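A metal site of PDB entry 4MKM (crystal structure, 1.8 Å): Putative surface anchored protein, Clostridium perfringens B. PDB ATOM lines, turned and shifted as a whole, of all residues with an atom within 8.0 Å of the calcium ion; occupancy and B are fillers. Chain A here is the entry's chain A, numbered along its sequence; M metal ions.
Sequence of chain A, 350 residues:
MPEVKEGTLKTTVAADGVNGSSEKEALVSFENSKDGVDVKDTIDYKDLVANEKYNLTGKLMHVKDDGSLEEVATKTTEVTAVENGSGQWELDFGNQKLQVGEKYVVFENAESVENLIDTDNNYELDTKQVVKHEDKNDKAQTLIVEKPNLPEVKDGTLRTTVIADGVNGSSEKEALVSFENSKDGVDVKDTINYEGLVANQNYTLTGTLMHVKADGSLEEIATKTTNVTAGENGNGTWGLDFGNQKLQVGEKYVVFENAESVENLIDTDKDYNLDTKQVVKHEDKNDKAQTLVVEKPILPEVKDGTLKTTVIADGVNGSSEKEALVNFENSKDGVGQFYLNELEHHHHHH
The side-chain carboxylate (OD1) of Asp 126 sits at hydrogen-bond distance from the side-chain hydroxyl (OG1) of Thr 119. O of Ile 117 is in hydrogen-bond range of N of Asp 126, at 2.9 Å. The side-chain carboxylate (OD1) of Asp 126 sits at hydrogen-bond distance from the side-chain hydroxyl (OG1) of Thr 127, at 3.3 Å. The side-chain carboxylate (OD2) of Asp 118 sits at hydrogen-bond distance from the backbone NH (N) of Tyr 123, 3.0 Å away.
Of the 11 residues printed, 5 come within 4 Å of the calcium ion.
The calcium ion is bound by the side-chain carboxylate (OD1) of Asp 120 (2.1 Å), the backbone carbonyl oxygen (O) of Glu 124 (2.2 Å), the side-chain carboxylate (OD2) of Asp 126 (2.2 Å), the side-chain carboxylate (OD1) of Asp 118 (2.3 Å) and the side-chain amide oxygen (OD1) of Asn 122 (2.5 Å). The calcium ion has five donor atoms within binding distance.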
ATOM      1  N   ILE A 117      26.890 -19.036  19.445  1.00  0.00           N
ATOM      2  CA  ILE A 117      26.616 -19.525  18.092  1.00  0.00           C
ATOM      3  C   ILE A 117      25.927 -20.882  18.128  1.00  0.00           C
ATOM      4  O   ILE A 117      26.346 -21.778  18.884  1.00  0.00           O
ATOM      5  CB  ILE A 117      27.948 -19.554  17.275  1.00  0.00           C
ATOM      6  CG1 ILE A 117      28.479 -18.109  17.045  1.00  0.00           C
ATOM      7  CG2 ILE A 117      27.774 -20.286  15.917  1.00  0.00           C
ATOM      8  CD1 ILE A 117      29.780 -18.047  16.533  1.00  0.00           C
ATOM      9  N   ASP A 118      24.911 -21.019  17.274  1.00  0.00           N
ATOM     10  CA  ASP A 118      24.200 -22.245  17.006  1.00  0.00           C
ATOM     11  C   ASP A 118      24.773 -22.806  15.686  1.00  0.00           C
ATOM     12  O   ASP A 118      24.549 -22.210  14.643  1.00  0.00           O
ATOM     13  CB  ASP A 118      22.703 -21.975  16.855  1.00  0.00           C
ATOM     14  CG  ASP A 118      21.878 -23.223  16.598  1.00  0.00           C
ATOM     15  OD1 ASP A 118      22.352 -24.348  16.941  1.00  0.00           O
ATOM     16  OD2 ASP A 118      20.769 -23.092  16.033  1.00  0.00           O
ATOM     17  N   THR A 119      25.494 -23.924  15.758  1.00  0.00           N
ATOM     18  CA  THR A 119      26.131 -24.580  14.600  1.00  0.00           C
ATOM     19  C   THR A 119      25.351 -25.770  14.019  1.00  0.00           C
ATOM     20  O   THR A 119      25.831 -26.361  13.055  1.00  0.00           O
ATOM     21  CB  THR A 119      27.533 -25.074  14.992  1.00  0.00           C
ATOM     22  OG1 THR A 119      27.391 -25.983  16.101  1.00  0.00           O
ATOM     23  CG2 THR A 119      28.469 -23.958  15.308  1.00  0.00           C
ATOM     24  N   ASP A 120      24.183 -26.155  14.600  1.00  0.00           N
ATOM     25  CA  ASP A 120      23.392 -27.306  14.133  1.00  0.00           C
ATOM     26  C   ASP A 120      21.894 -27.022  13.947  1.00  0.00           C
ATOM     27  O   ASP A 120      21.095 -27.964  13.890  1.00  0.00           O
ATOM     28  CB  ASP A 120      23.642 -28.532  15.051  1.00  0.00           C
ATOM     29  CG  ASP A 120      23.096 -28.406  16.454  1.00  0.00           C
ATOM     30  OD1 ASP A 120      23.097 -27.274  16.997  1.00  0.00           O
ATOM     31  OD2 ASP A 120      22.696 -29.441  17.017  1.00  0.00           O
ATOM     32  N   ASN A 121      21.509 -25.735  13.803  1.00  0.00           N
ATOM     33  CA  ASN A 121      20.130 -25.313  13.534  1.00  0.00           C
ATOM     34  C   ASN A 121      19.017 -25.898  14.448  1.00  0.00           C
ATOM     35  O   ASN A 121      17.956 -26.282  13.936  1.00  0.00           O
ATOM     36  CB  ASN A 121      19.787 -25.519  12.044  1.00  0.00           C
ATOM     37  N   ASN A 122      19.234 -25.902  15.781  1.00  0.00           N
ATOM     38  CA  ASN A 122      18.219 -26.346  16.755  1.00  0.00           C
ATOM     39  C   ASN A 122      17.835 -25.212  17.737  1.00  0.00           C
ATOM     40  O   ASN A 122      17.126 -25.484  18.710  1.00  0.00           O
ATOM     41  CB  ASN A 122      18.689 -27.598  17.514  1.00  0.00           C
ATOM     42  CG  ASN A 122      19.929 -27.406  18.362  1.00  0.00           C
ATOM     43  OD1 ASN A 122      20.404 -26.290  18.556  1.00  0.00           O
ATOM     44  ND2 ASN A 122      20.436 -28.482  18.931  1.00  0.00           N
ATOM     45  N   TYR A 123      18.291 -23.973  17.506  1.00  0.00           N
ATOM     46  CA  TYR A 123      18.071 -22.787  18.347  1.00  0.00           C
ATOM     47  C   TYR A 123      18.782 -22.882  19.714  1.00  0.00           C
ATOM     48  O   TYR A 123      18.637 -21.962  20.523  1.00  0.00           O
ATOM     49  CB  TYR A 123      16.585 -22.451  18.530  1.00  0.00           C
ATOM     50  CG  TYR A 123      15.891 -22.077  17.247  1.00  0.00           C
ATOM     51  CD1 TYR A 123      16.064 -20.821  16.689  1.00  0.00           C
ATOM     52  CD2 TYR A 123      15.000 -22.954  16.642  1.00  0.00           C
ATOM     53  CE1 TYR A 123      15.359 -20.441  15.538  1.00  0.00           C
ATOM     54  CE2 TYR A 123      14.320 -22.598  15.478  1.00  0.00           C
ATOM     55  CZ  TYR A 123      14.486 -21.326  14.947  1.00  0.00           C
ATOM     56  OH  TYR A 123      13.839 -20.947  13.788  1.00  0.00           O
ATOM     57  N   GLU A 124      19.574 -23.928  19.966  1.00  0.00           N
ATOM     58  CA  GLU A 124      20.272 -24.061  21.228  1.00  0.00           C
ATOM     59  C   GLU A 124      21.725 -23.695  20.882  1.00  0.00           C
ATOM     60  O   GLU A 124      22.379 -24.387  20.075  1.00  0.00           O
ATOM     61  CB  GLU A 124      20.181 -25.472  21.788  1.00  0.00           C
ATOM     62  CG  GLU A 124      18.756 -25.981  22.038  1.00  0.00           C
ATOM     63  CD  GLU A 124      18.157 -25.661  23.389  1.00  0.00           C
ATOM     64  OE1 GLU A 124      18.697 -24.802  24.118  1.00  0.00           O
ATOM     65  OE2 GLU A 124      17.104 -26.266  23.710  1.00  0.00           O
ATOM     66  N   LEU A 125      22.242 -22.674  21.547  1.00  0.00           N
ATOM     67  CA  LEU A 125      23.591 -22.174  21.306  1.00  0.00           C
ATOM     68  C   LEU A 125      24.657 -23.172  21.836  1.00  0.00           C
ATOM     69  O   LEU A 125      24.516 -23.675  22.954  1.00  0.00           O
ATOM     70  CB  LEU A 125      23.759 -20.777  21.932  1.00  0.00           C
ATOM     71  CG  LEU A 125      22.698 -19.729  21.606  1.00  0.00           C
ATOM     72  CD1 LEU A 125      22.994 -18.417  22.290  1.00  0.00           C
ATOM     73  CD2 LEU A 125      22.594 -19.516  20.109  1.00  0.00           C
ATOM     74  N   ASP A 126      25.653 -23.538  21.021  1.00  0.00           N
ATOM     75  CA  ASP A 126      26.638 -24.598  21.346  1.00  0.00           C
ATOM     76  C   ASP A 126      28.134 -24.287  21.181  1.00  0.00           C
ATOM     77  O   ASP A 126      28.961 -25.145  21.500  1.00  0.00           O
ATOM     78  CB  ASP A 126      26.291 -25.821  20.492  1.00  0.00           C
ATOM     79  CG  ASP A 126      26.172 -25.500  19.018  1.00  0.00           C
ATOM     80  OD1 ASP A 126      27.185 -25.138  18.407  1.00  0.00           O
ATOM     81  OD2 ASP A 126      25.052 -25.498  18.497  1.00  0.00           O
ATOM     82  N   THR A 127      28.495 -23.124  20.645  1.00  0.00           N
ATOM     83  CA  THR A 127      29.888 -22.756  20.399  1.00  0.00           C
ATOM     84  C   THR A 127      30.123 -21.264  20.693  1.00  0.00           C
ATOM     85  O   THR A 127      29.221 -20.436  20.482  1.00  0.00           O
ATOM     86  CB  THR A 127      30.328 -23.138  18.975  1.00  0.00           C
ATOM     87  OG1 THR A 127      29.399 -22.657  18.037  1.00  0.00           O
ATOM     88  CG2 THR A 127      30.493 -24.649  18.786  1.00  0.00           C
HETATM   89 CA    CA M   1      22.860 -25.940  18.564  1.00  0.00          CA
